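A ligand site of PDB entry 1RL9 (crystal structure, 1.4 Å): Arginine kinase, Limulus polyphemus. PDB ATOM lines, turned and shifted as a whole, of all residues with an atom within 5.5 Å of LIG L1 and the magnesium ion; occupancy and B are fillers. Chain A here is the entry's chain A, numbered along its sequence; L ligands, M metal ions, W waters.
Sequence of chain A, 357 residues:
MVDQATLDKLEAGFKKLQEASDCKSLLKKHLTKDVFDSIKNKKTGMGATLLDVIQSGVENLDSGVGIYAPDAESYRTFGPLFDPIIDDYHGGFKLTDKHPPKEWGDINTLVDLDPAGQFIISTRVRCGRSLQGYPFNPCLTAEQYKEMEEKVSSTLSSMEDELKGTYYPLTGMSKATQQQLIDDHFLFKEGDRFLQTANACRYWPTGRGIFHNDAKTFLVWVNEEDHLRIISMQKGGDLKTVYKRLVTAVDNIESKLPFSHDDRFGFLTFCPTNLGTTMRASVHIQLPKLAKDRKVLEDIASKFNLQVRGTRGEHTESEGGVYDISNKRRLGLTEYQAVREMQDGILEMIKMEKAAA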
ATOM      1  N   SER A 122       7.730  11.471 -22.541  1.00  0.00           N
ATOM      2  CA  SER A 122       7.399  11.928 -23.871  1.00  0.00           C
ATOM      3  C   SER A 122       6.293  12.995 -23.786  1.00  0.00           C
ATOM      4  O   SER A 122       5.537  13.039 -22.809  1.00  0.00           O
ATOM      5  CB  SER A 122       6.968  10.720 -24.713  1.00  0.00           C
ATOM      6  OG  SER A 122       5.871  10.068 -24.101  1.00  0.00           O
ATOM      7  N   THR A 123       6.176  13.798 -24.848  1.00  0.00           N
ATOM      8  CA  THR A 123       5.280  14.949 -24.879  1.00  0.00           C
ATOM      9  C   THR A 123       4.492  14.893 -26.147  1.00  0.00           C
ATOM     10  O   THR A 123       5.003  14.589 -27.200  1.00  0.00           O
ATOM     11  CB  THR A 123       6.167  16.235 -24.792  1.00  0.00           C
ATOM     12  OG1 THR A 123       6.985  16.182 -23.617  1.00  0.00           O
ATOM     13  CG2 THR A 123       5.311  17.485 -24.712  1.00  0.00           C
ATOM     14  N   ARG A 124       3.235  15.297 -26.035  1.00  0.00           N
ATOM     15  CA  ARG A 124       2.321  15.255 -27.176  1.00  0.00           C
ATOM     16  C   ARG A 124       1.304  16.347 -27.116  1.00  0.00           C
ATOM     17  O   ARG A 124       0.839  16.674 -26.035  1.00  0.00           O
ATOM     18  CB  ARG A 124       1.590  13.884 -27.162  1.00  0.00           C
ATOM     19  CG  ARG A 124       0.536  13.584 -28.268  1.00  0.00           C
ATOM     20  CD  ARG A 124       0.120  12.155 -28.062  1.00  0.00           C
ATOM     21  NE  ARG A 124      -0.849  11.616 -29.016  1.00  0.00           N
ATOM     22  CZ  ARG A 124      -2.171  11.726 -28.931  1.00  0.00           C
ATOM     23  NH1 ARG A 124      -2.733  12.402 -27.931  1.00  0.00           N
ATOM     24  NH2 ARG A 124      -2.969  11.021 -29.778  1.00  0.00           N
ATOM     25  N   ARG A 126      -2.296  17.425 -29.320  1.00  0.00           N
ATOM     26  CA  ARG A 126      -3.148  17.163 -30.443  1.00  0.00           C
ATOM     27  C   ARG A 126      -4.332  18.118 -30.454  1.00  0.00           C
ATOM     28  O   ARG A 126      -4.740  18.697 -29.428  1.00  0.00           O
ATOM     29  CB  ARG A 126      -3.688  15.696 -30.410  1.00  0.00           C
ATOM     30  CG  ARG A 126      -4.600  15.299 -29.227  1.00  0.00           C
ATOM     31  CD  ARG A 126      -6.054  15.740 -29.325  1.00  0.00           C
ATOM     32  NE  ARG A 126      -6.867  14.975 -28.358  1.00  0.00           N
ATOM     33  CZ  ARG A 126      -8.015  15.423 -27.876  1.00  0.00           C
ATOM     34  NH1 ARG A 126      -8.707  14.691 -27.055  1.00  0.00           N
ATOM     35  NH2 ARG A 126      -8.463  16.639 -28.225  1.00  0.00           N
ATOM     36  N   ILE A 182       0.064   0.988 -32.334  1.00  0.00           N
ATOM     37  CA  ILE A 182      -0.706   1.303 -31.125  1.00  0.00           C
ATOM     38  C   ILE A 182       0.225   1.129 -29.940  1.00  0.00           C
ATOM     39  O   ILE A 182       0.241   1.987 -29.036  1.00  0.00           O
ATOM     40  CB  ILE A 182      -1.915   0.318 -30.987  1.00  0.00           C
ATOM     41  CG1 ILE A 182      -2.872   0.554 -32.143  1.00  0.00           C
ATOM     42  CG2 ILE A 182      -2.628   0.458 -29.635  1.00  0.00           C
ATOM     43  CD1 ILE A 182      -4.018  -0.545 -32.234  1.00  0.00           C
ATOM     44  N   HIS A 185       2.253   4.065 -29.276  1.00  0.00           N
ATOM     45  CA  HIS A 185       1.456   5.260 -28.925  1.00  0.00           C
ATOM     46  C   HIS A 185       1.135   6.220 -30.059  1.00  0.00           C
ATOM     47  O   HIS A 185       0.689   7.339 -29.797  1.00  0.00           O
ATOM     48  CB  HIS A 185       2.146   6.028 -27.789  1.00  0.00           C
ATOM     49  CG  HIS A 185       2.549   5.171 -26.636  1.00  0.00           C
ATOM     50  ND1 HIS A 185       1.650   4.462 -25.861  1.00  0.00           N
ATOM     51  CD2 HIS A 185       3.773   4.855 -26.152  1.00  0.00           C
ATOM     52  CE1 HIS A 185       2.310   3.761 -24.947  1.00  0.00           C
ATOM     53  NE2 HIS A 185       3.591   3.985 -25.105  1.00  0.00           N
ATOM     54  N   PHE A 186       1.288   5.753 -31.291  1.00  0.00           N
ATOM     55  CA  PHE A 186       1.067   6.585 -32.471  1.00  0.00           C
ATOM     56  C   PHE A 186      -0.324   6.488 -33.054  1.00  0.00           C
ATOM     57  O   PHE A 186      -0.928   7.485 -33.360  1.00  0.00           O
ATOM     58  CB  PHE A 186       2.092   6.204 -33.563  1.00  0.00           C
ATOM     59  CG  PHE A 186       3.505   6.474 -33.170  1.00  0.00           C
ATOM     60  CD1 PHE A 186       4.454   5.455 -33.214  1.00  0.00           C
ATOM     61  CD2 PHE A 186       3.882   7.721 -32.731  1.00  0.00           C
ATOM     62  CE1 PHE A 186       5.764   5.693 -32.805  1.00  0.00           C
ATOM     63  CE2 PHE A 186       5.199   7.966 -32.325  1.00  0.00           C
ATOM     64  CZ  PHE A 186       6.140   6.946 -32.358  1.00  0.00           C
ATOM     65  N   LEU A 187      -0.822   5.284 -33.170  1.00  0.00           N
ATOM     66  CA  LEU A 187      -2.098   4.989 -33.800  1.00  0.00           C
ATOM     67  C   LEU A 187      -3.222   4.731 -32.785  1.00  0.00           C
ATOM     68  O   LEU A 187      -3.003   4.104 -31.746  1.00  0.00           O
ATOM     69  CB  LEU A 187      -1.926   3.720 -34.654  1.00  0.00           C
ATOM     70  CG  LEU A 187      -3.148   3.189 -35.402  1.00  0.00           C
ATOM     71  CD1 LEU A 187      -3.593   4.214 -36.476  1.00  0.00           C
ATOM     72  CD2 LEU A 187      -2.749   1.878 -36.051  1.00  0.00           C
ATOM     73  N   TRP A 221      -4.737  11.432 -37.613  1.00  0.00           N
ATOM     74  CA  TRP A 221      -5.666  10.285 -37.616  1.00  0.00           C
ATOM     75  C   TRP A 221      -6.864  10.708 -38.462  1.00  0.00           C
ATOM     76  O   TRP A 221      -7.403  11.817 -38.256  1.00  0.00           O
ATOM     77  CB  TRP A 221      -6.207  10.005 -36.246  1.00  0.00           C
ATOM     78  CG  TRP A 221      -5.200   9.517 -35.221  1.00  0.00           C
ATOM     79  CD1 TRP A 221      -3.903   9.043 -35.413  1.00  0.00           C
ATOM     80  CD2 TRP A 221      -5.479   9.344 -33.842  1.00  0.00           C
ATOM     81  NE1 TRP A 221      -3.401   8.596 -34.218  1.00  0.00           N
ATOM     82  CE2 TRP A 221      -4.345   8.765 -33.229  1.00  0.00           C
ATOM     83  CE3 TRP A 221      -6.601   9.630 -33.051  1.00  0.00           C
ATOM     84  CZ2 TRP A 221      -4.295   8.468 -31.841  1.00  0.00           C
ATOM     85  CZ3 TRP A 221      -6.548   9.341 -31.679  1.00  0.00           C
ATOM     86  CH2 TRP A 221      -5.408   8.770 -31.106  1.00  0.00           C
ATOM     87  N   GLU A 224     -11.326   8.560 -36.958  1.00  0.00           N
ATOM     88  CA  GLU A 224     -11.535   7.818 -35.734  1.00  0.00           C
ATOM     89  C   GLU A 224     -12.657   8.589 -35.010  1.00  0.00           C
ATOM     90  O   GLU A 224     -13.740   8.749 -35.565  1.00  0.00           O
ATOM     91  CB  GLU A 224     -10.235   7.725 -34.866  1.00  0.00           C
ATOM     92  CG  GLU A 224     -10.381   6.780 -33.623  1.00  0.00           C
ATOM     93  CD  GLU A 224     -10.028   7.411 -32.285  1.00  0.00           C
ATOM     94  OE1 GLU A 224     -10.124   8.640 -32.170  1.00  0.00           O
ATOM     95  OE2 GLU A 224      -9.663   6.653 -31.356  1.00  0.00           O
ATOM     96  N   GLU A 225     -12.441   9.115 -33.806  1.00  0.00           N
ATOM     97  CA  GLU A 225     -13.497   9.817 -33.089  1.00  0.00           C
ATOM     98  C   GLU A 225     -13.937  11.101 -33.825  1.00  0.00           C
ATOM     99  O   GLU A 225     -15.141  11.384 -33.915  1.00  0.00           O
ATOM    100  CB  GLU A 225     -12.987  10.163 -31.690  1.00  0.00           C
ATOM    101  CG  GLU A 225     -14.055  10.775 -30.798  1.00  0.00           C
ATOM    102  CD  GLU A 225     -13.576  10.995 -29.431  1.00  0.00           C
ATOM    103  OE1 GLU A 225     -13.992  12.003 -28.844  1.00  0.00           O
ATOM    104  OE2 GLU A 225     -12.793  10.155 -28.899  1.00  0.00           O
ATOM    105  N   ARG A 229      -7.682  14.130 -36.349  1.00  0.00           N
ATOM    106  CA  ARG A 229      -6.952  14.466 -35.136  1.00  0.00           C
ATOM    107  C   ARG A 229      -5.551  14.793 -35.663  1.00  0.00           C
ATOM    108  O   ARG A 229      -4.905  13.953 -36.310  1.00  0.00           O
ATOM    109  CB  ARG A 229      -6.888  13.336 -34.137  1.00  0.00           C
ATOM    110  CG  ARG A 229      -8.191  13.123 -33.452  1.00  0.00           C
ATOM    111  CD  ARG A 229      -8.518  14.243 -32.469  1.00  0.00           C
ATOM    112  NE  ARG A 229      -9.761  13.920 -31.753  1.00  0.00           N
ATOM    113  CZ  ARG A 229      -9.847  13.092 -30.718  1.00  0.00           C
ATOM    114  NH1 ARG A 229      -8.764  12.497 -30.246  1.00  0.00           N
ATOM    115  NH2 ARG A 229     -11.025  12.835 -30.153  1.00  0.00           N
ATOM    116  N   MET A 233       4.191  14.938 -31.602  1.00  0.00           N
ATOM    117  CA  MET A 233       4.713  14.288 -30.395  1.00  0.00           C
ATOM    118  C   MET A 233       6.142  13.829 -30.600  1.00  0.00           C
ATOM    119  O   MET A 233       6.576  13.625 -31.716  1.00  0.00           O
ATOM    120  CB  MET A 233       3.847  13.069 -30.008  1.00  0.00           C
ATOM    121  CG  MET A 233       3.767  12.012 -31.095  1.00  0.00           C
ATOM    122  SD  MET A 233       2.455  10.730 -30.833  1.00  0.00           S
ATOM    123  CE  MET A 233       3.200   9.745 -29.570  1.00  0.00           C
ATOM    124  N   ARG A 280      -5.479  18.886 -26.571  1.00  0.00           N
ATOM    125  CA  ARG A 280      -5.064  18.066 -25.452  1.00  0.00           C
ATOM    126  C   ARG A 280      -3.533  17.963 -25.497  1.00  0.00           C
ATOM    127  O   ARG A 280      -2.973  17.321 -26.388  1.00  0.00           O
ATOM    128  CB  ARG A 280      -5.689  16.682 -25.473  1.00  0.00           C
ATOM    129  CG  ARG A 280      -5.481  15.944 -24.116  1.00  0.00           C
ATOM    130  CD  ARG A 280      -6.291  14.666 -24.005  1.00  0.00           C
ATOM    131  NE  ARG A 280      -5.648  13.455 -24.524  1.00  0.00           N
ATOM    132  CZ  ARG A 280      -4.700  12.796 -23.866  1.00  0.00           C
ATOM    133  NH1 ARG A 280      -4.270  13.223 -22.697  1.00  0.00           N
ATOM    134  NH2 ARG A 280      -4.210  11.668 -24.366  1.00  0.00           N
ATOM    135  N   SER A 282      -0.263  16.732 -23.521  1.00  0.00           N
ATOM    136  CA  SER A 282       0.006  15.786 -22.465  1.00  0.00           C
ATOM    137  C   SER A 282       1.457  15.419 -22.354  1.00  0.00           C
ATOM    138  O   SER A 282       2.253  15.615 -23.274  1.00  0.00           O
ATOM    139  CB  SER A 282      -0.761  14.475 -22.685  1.00  0.00           C
ATOM    140  OG  SER A 282      -2.129  14.682 -22.920  1.00  0.00           O
ATOM    141  N   VAL A 283       1.778  14.856 -21.185  1.00  0.00           N
ATOM    142  CA  VAL A 283       3.091  14.246 -21.002  1.00  0.00           C
ATOM    143  C   VAL A 283       2.861  12.830 -20.465  1.00  0.00           C
ATOM    144  O   VAL A 283       1.857  12.563 -19.772  1.00  0.00           O
ATOM    145  CB  VAL A 283       4.004  14.988 -19.970  1.00  0.00           C
ATOM    146  CG1 VAL A 283       4.525  16.293 -20.536  1.00  0.00           C
ATOM    147  CG2 VAL A 283       3.235  15.223 -18.675  1.00  0.00           C
ATOM    148  N   HIS A 284       3.744  11.920 -20.828  1.00  0.00           N
ATOM    149  CA  HIS A 284       3.850  10.629 -20.150  1.00  0.00           C
ATOM    150  C   HIS A 284       4.907  10.945 -19.113  1.00  0.00           C
ATOM    151  O   HIS A 284       6.019  11.373 -19.438  1.00  0.00           O
ATOM    152  CB  HIS A 284       4.326   9.543 -21.084  1.00  0.00           C
ATOM    153  CG  HIS A 284       3.199   8.861 -21.793  1.00  0.00           C
ATOM    154  ND1 HIS A 284       3.347   7.719 -22.540  1.00  0.00           N
ATOM    155  CD2 HIS A 284       1.876   9.175 -21.850  1.00  0.00           C
ATOM    156  CE1 HIS A 284       2.172   7.359 -23.031  1.00  0.00           C
ATOM    157  NE2 HIS A 284       1.263   8.221 -22.630  1.00  0.00           N
ATOM    158  N   ARG A 309      -4.699   9.869 -17.303  1.00  0.00           N
ATOM    159  CA  ARG A 309      -5.085   8.705 -18.106  1.00  0.00           C
ATOM    160  C   ARG A 309      -3.976   7.661 -17.979  1.00  0.00           C
ATOM    161  O   ARG A 309      -2.835   7.965 -17.637  1.00  0.00           O
ATOM    162  CB  ARG A 309      -5.264   9.069 -19.593  1.00  0.00           C
ATOM    163  CG  ARG A 309      -6.435  10.054 -19.836  1.00  0.00           C
ATOM    164  CD  ARG A 309      -6.472  10.477 -21.314  1.00  0.00           C
ATOM    165  NE  ARG A 309      -7.549  11.453 -21.465  1.00  0.00           N
ATOM    166  CZ  ARG A 309      -8.190  11.709 -22.584  1.00  0.00           C
ATOM    167  NH1 ARG A 309      -7.914  11.068 -23.676  1.00  0.00           N
ATOM    168  NH2 ARG A 309      -9.114  12.663 -22.614  1.00  0.00           N
ATOM    169  N   GLY A 310      -4.296   6.429 -18.371  1.00  0.00           N
ATOM    170  CA  GLY A 310      -3.303   5.345 -18.368  1.00  0.00           C
ATOM    171  C   GLY A 310      -2.276   5.509 -19.494  1.00  0.00           C
ATOM    172  O   GLY A 310      -2.400   6.388 -20.367  1.00  0.00           O
ATOM    173  N   THR A 311      -1.268   4.645 -19.508  1.00  0.00           N
ATOM    174  CA  THR A 311      -0.212   4.738 -20.489  1.00  0.00           C
ATOM    175  C   THR A 311      -0.667   4.557 -21.925  1.00  0.00           C
ATOM    176  O   THR A 311      -0.110   5.148 -22.845  1.00  0.00           O
ATOM    177  CB  THR A 311       0.891   3.701 -20.177  1.00  0.00           C
ATOM    178  OG1 THR A 311       1.100   3.700 -18.760  1.00  0.00           O
ATOM    179  CG2 THR A 311       2.221   4.023 -20.950  1.00  0.00           C
ATOM    180  N   ARG A 312      -1.718   3.755 -22.129  1.00  0.00           N
ATOM    181  CA  ARG A 312      -2.223   3.510 -23.472  1.00  0.00           C
ATOM    182  C   ARG A 312      -3.434   4.371 -23.774  1.00  0.00           C
ATOM    183  O   ARG A 312      -4.168   4.133 -24.774  1.00  0.00           O
ATOM    184  CB  ARG A 312      -2.536   2.012 -23.659  1.00  0.00           C
ATOM    185  CG  ARG A 312      -1.270   1.139 -23.532  1.00  0.00           C
ATOM    186  CD  ARG A 312      -1.536  -0.354 -23.799  1.00  0.00           C
ATOM    187  NE  ARG A 312      -1.659  -0.524 -25.249  1.00  0.00           N
ATOM    188  CZ  ARG A 312      -1.617  -1.678 -25.909  1.00  0.00           C
ATOM    189  NH1 ARG A 312      -1.450  -2.827 -25.264  1.00  0.00           N
ATOM    190  NH2 ARG A 312      -1.740  -1.675 -27.230  1.00  0.00           N
ATOM    191  N   GLY A 313      -3.617   5.386 -22.928  1.00  0.00           N
ATOM    192  CA  GLY A 313      -4.699   6.325 -23.140  1.00  0.00           C
ATOM    193  C   GLY A 313      -5.831   6.203 -22.176  1.00  0.00           C
ATOM    194  O   GLY A 313      -5.754   5.466 -21.185  1.00  0.00           O
ATOM    195  N   GLU A 314      -6.891   6.948 -22.428  1.00  0.00           N
ATOM    196  CA  GLU A 314      -8.038   6.871 -21.555  1.00  0.00           C
ATOM    197  C   GLU A 314      -8.586   5.424 -21.465  1.00  0.00           C
ATOM    198  O   GLU A 314      -8.505   4.615 -22.396  1.00  0.00           O
ATOM    199  CB  GLU A 314      -9.148   7.820 -22.052  1.00  0.00           C
ATOM    200  CG  GLU A 314      -9.578   7.487 -23.459  1.00  0.00           C
ATOM    201  CD  GLU A 314     -10.810   8.284 -23.854  1.00  0.00           C
ATOM    202  OE1 GLU A 314     -11.268   9.116 -23.031  1.00  0.00           O
ATOM    203  OE2 GLU A 314     -11.295   8.039 -24.992  1.00  0.00           O
ATOM    204  N   ASP A 324      -0.380   9.445 -18.134  1.00  0.00           N
ATOM    205  CA  ASP A 324      -0.634  10.457 -19.147  1.00  0.00           C
ATOM    206  C   ASP A 324      -1.335  11.567 -18.382  1.00  0.00           C
ATOM    207  O   ASP A 324      -2.418  11.374 -17.783  1.00  0.00           O
ATOM    208  CB  ASP A 324      -1.506   9.808 -20.267  1.00  0.00           C
ATOM    209  CG  ASP A 324      -2.206  10.793 -21.212  1.00  0.00           C
ATOM    210  OD1 ASP A 324      -2.392  11.994 -20.927  1.00  0.00           O
ATOM    211  OD2 ASP A 324      -2.629  10.290 -22.273  1.00  0.00           O
HETATM  212  P1  LIG L   1      -6.595  11.314 -27.553  1.00  0.00           P
HETATM  213  O1  LIG L   1      -7.614  10.523 -28.355  1.00  0.00           O
HETATM  214  O2  LIG L   1      -5.465  11.581 -28.418  1.00  0.00           O
HETATM  215  O3  LIG L   1      -7.136  12.401 -26.761  1.00  0.00           O
HETATM  216  P2  LIG L   1      -6.175   8.824 -25.926  1.00  0.00           P
HETATM  217  O4  LIG L   1      -7.252   8.188 -26.728  1.00  0.00           O
HETATM  218  O5  LIG L   1      -6.262   8.835 -24.491  1.00  0.00           O
HETATM  219  O6  LIG L   1      -5.947  10.317 -26.405  1.00  0.00           O
HETATM  220  O7  LIG L   1      -4.776   8.189 -26.310  1.00  0.00           O
HETATM  221  C1  LIG L   1      -4.449   8.156 -27.719  1.00  0.00           C
HETATM  222  C2  LIG L   1      -2.989   7.690 -27.807  1.00  0.00           C
HETATM  223  O8  LIG L   1      -2.117   8.777 -27.464  1.00  0.00           O
HETATM  224  C3  LIG L   1      -2.622   6.466 -26.917  1.00  0.00           C
HETATM  225  O9  LIG L   1      -1.775   5.562 -27.706  1.00  0.00           O
HETATM  226  C4  LIG L   1      -1.732   7.109 -25.874  1.00  0.00           C
HETATM  227  O10 LIG L   1      -0.742   6.264 -25.294  1.00  0.00           O
HETATM  228  C5  LIG L   1      -1.046   8.222 -26.674  1.00  0.00           C
HETATM  229  N1  LIG L   1      -0.445   9.316 -25.912  1.00  0.00           N
HETATM  230  C6  LIG L   1      -1.090  10.321 -25.228  1.00  0.00           C
HETATM  231  N2  LIG L   1      -0.265  11.215 -24.663  1.00  0.00           N
HETATM  232  C7  LIG L   1       0.996  10.708 -24.995  1.00  0.00           C
HETATM  233  C8  LIG L   1       2.266  11.245 -24.662  1.00  0.00           C
HETATM  234  N3  LIG L   1       2.519  12.332 -23.961  1.00  0.00           N
HETATM  235  N4  LIG L   1       3.307  10.517 -25.138  1.00  0.00           N
HETATM  236  C9  LIG L   1       3.133   9.368 -25.835  1.00  0.00           C
HETATM  237  N5  LIG L   1       1.941   8.918 -26.164  1.00  0.00           N
HETATM  238  C10 LIG L   1       0.866   9.579 -25.746  1.00  0.00           C
HETATM  239  N1  LG2 L   2     -13.526  10.232 -26.317  1.00  0.00           N
HETATM  240  C1  LG2 L   2     -13.636  11.101 -25.332  1.00  0.00           C
HETATM  241  N2  LG2 L   2     -13.525  12.402 -25.600  1.00  0.00           N
HETATM  242  N3  LG2 L   2     -13.878  10.740 -24.091  1.00  0.00           N
HETATM  243  C2  LG2 L   2     -13.998   9.350 -23.672  1.00  0.00           C
HETATM  244  C3  LG2 L   2     -14.232  11.761 -23.109  1.00  0.00           C
HETATM  245  C4  LG2 L   2     -15.691  12.169 -23.222  1.00  0.00           C
HETATM  246  O1  LG2 L   2     -16.488  11.356 -23.786  1.00  0.00           O
HETATM  247  O2  LG2 L   2     -16.035  13.268 -22.789  1.00  0.00           O
HETATM  248 MG    MG M   1      -8.799   8.885 -28.016  1.00  0.00          MG
HETATM  249  O   HOH W   1     -10.084   9.608 -29.483  1.00  0.00           O
HETATM  250  O   HOH W   2     -10.122   7.426 -27.394  1.00  0.00           O
HETATM  251  O   HOH W   3      -7.735   5.461 -26.689  1.00  0.00           O
HETATM  252  O   HOH W   4      -9.670  10.067 -26.511  1.00  0.00           O
HETATM  253  O   HOH W   5      -5.964  12.518 -30.936  1.00  0.00           O
HETATM  254  O   HOH W   6      -1.583   7.825 -22.808  1.00  0.00           O
HETATM  255  O   HOH W   7      -0.922   3.143 -26.725  1.00  0.00           O
HETATM  256  O   HOH W   8      -3.795   4.345 -29.110  1.00  0.00           O
HETATM  257  O   HOH W   9      -8.087   7.533 -29.414  1.00  0.00           O
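O5 of LIG L1 sits at hydrogen-bond distance from N of Glu 314 (2.9 Å).
A nitrogen (N1) of LG2 L2 is in salt-bridge range of the side-chain carboxylate (OE2) of Glu 225 (2.7 Å).
O of Thr 311 lies within hydrogen-bond range of O10 of LIG L1.
The backbone carbonyl oxygen (O) of Ser 282 sits at hydrogen-bond distance from a nitrogen (N3) of LIG L1 (3.4 Å).
N4 of LIG L1 is in hydrogen-bond range of OG of Ser 122.
A nitrogen (N3) of LIG L1 lies within hydrogen-bond range of the backbone carbonyl oxygen (O) of Ser 122, 3.3 Å away.
A nitrogen (N3) of LG2 L2 lies within salt-bridge range of the side-chain carboxylate of Glu 314 (3.3 Å).
An oxygen (O10) of LIG L1 sits at hydrogen-bond distance from a ring nitrogen (ND1) of His 185 (3.0 Å).
The guanidinium group of Arg 309 is in salt-bridge range of an oxygen (O5) of LIG L1, at 2.9 Å.
The guanidinium group of Arg 126 is in salt-bridge range of an oxygen (O3) of LIG L1 (2.8 Å).
NH1 of Arg 124 lies within salt-bridge range of O2 of LIG L1, 2.9 Å away.
O3 of LIG L1 is in salt-bridge range of NE of Arg 280 (2.9 Å).
The guanidinium group (NH1) of Arg 229 lies within salt-bridge range of an oxygen (O3) of LIG L1 (3.8 Å).
The backbone carbonyl oxygen of Arg 126 is in hydrogen-bond range of the backbone NH of Arg 280 (3.0 Å).
The backbone NH (N) of Arg 309 sits at hydrogen-bond distance from the backbone carbonyl oxygen (O) of Asp 324, at 2.8 Å.
NE1 of Trp 221 is in hydrogen-bond range of O of Phe 186 (2.8 Å).
O of Arg 124 sits at hydrogen-bond distance from N of Ser 282, at 2.7 Å.
The backbone carbonyl oxygen (O) of Ser 122 lies within hydrogen-bond range of the backbone NH (N) of His 284 (2.9 Å).
The backbone carbonyl oxygen (O) of Arg 229 sits at hydrogen-bond distance from the backbone NH (N) of Trp 221, 2.8 Å away.
NH1 of Arg 280 is in hydrogen-bond range of OG of Ser 282 (2.6 Å).
The guanidinium group (NH1) of Arg 280 is in salt-bridge range of the side-chain carboxylate (OD1) of Asp 324, 2.9 Å away.
N of His 284 sits close to N3 of LIG L1, 3.4 Å away.
OD2 of Asp 324 sits close to N2 of LIG L1 (3.5 Å).
Thr 123 touches LIG L1 (C to N3, 3.9 Å).
Trp 221 touches LIG L1.
CE of Met 233 touches N5 of LIG L1, 3.7 Å away.
C of Val 283 touches N3 of LIG L1, 3.5 Å away.
Arg 312 touches LIG L1 (O to C3, 3.5 Å).
Gly 313 touches LIG L1.
Hydrophobic or aromatic side chains that line LIG L1: His 185, Trp 221, Met 233 and His 284.
Of the 24 residues printed, 18 come within 4 Å of LIG L1.
No residue comes within 4 Å of the magnesium ion.
The nearest printed residue that does not touch the magnesium ion is Glu 314 (4.01 Å).
O1 of LIG L1 is bound to the magnesium ion, at 2.0 Å.
Water W2 binds the magnesium ion, at 2.1 Å.
Water W9 is bound to the magnesium ion, 2.1 Å away.
Water W1 binds the magnesium ion, at 2.1 Å.
The magnesium ion is bound by water W4, 2.1 Å away.
O4 of LIG L1 is bound to the magnesium ion.
Water W1 lies within hydrogen-bond range of the side-chain carboxylate of Glu 225 (2.8 Å), the side-chain carboxylate of Glu 224 (2.9 Å) and the guanidinium group of Arg 229 (3.3 Å).
Water W4 lies within hydrogen-bond range of OE2 of Glu 314 (3.0 Å), O3 of LIG L1 (3.5 Å) and NH1 of Arg 309 (3.5 Å).
Water W5 lies within hydrogen-bond range of an oxygen (O2) of LIG L1 (2.7 Å) and the guanidinium group of Arg 229 (2.9 Å).
Water W8 lies within hydrogen-bond range of O9 of LIG L1 (2.7 Å) and O of Leu 187 (2.8 Å).
Water W7 lies within hydrogen-bond range of an oxygen (O9) of LIG L1 (2.7 Å), the backbone carbonyl oxygen of Ile 182 (2.8 Å) and a ring nitrogen (ND1) of His 185 (3.0 Å).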
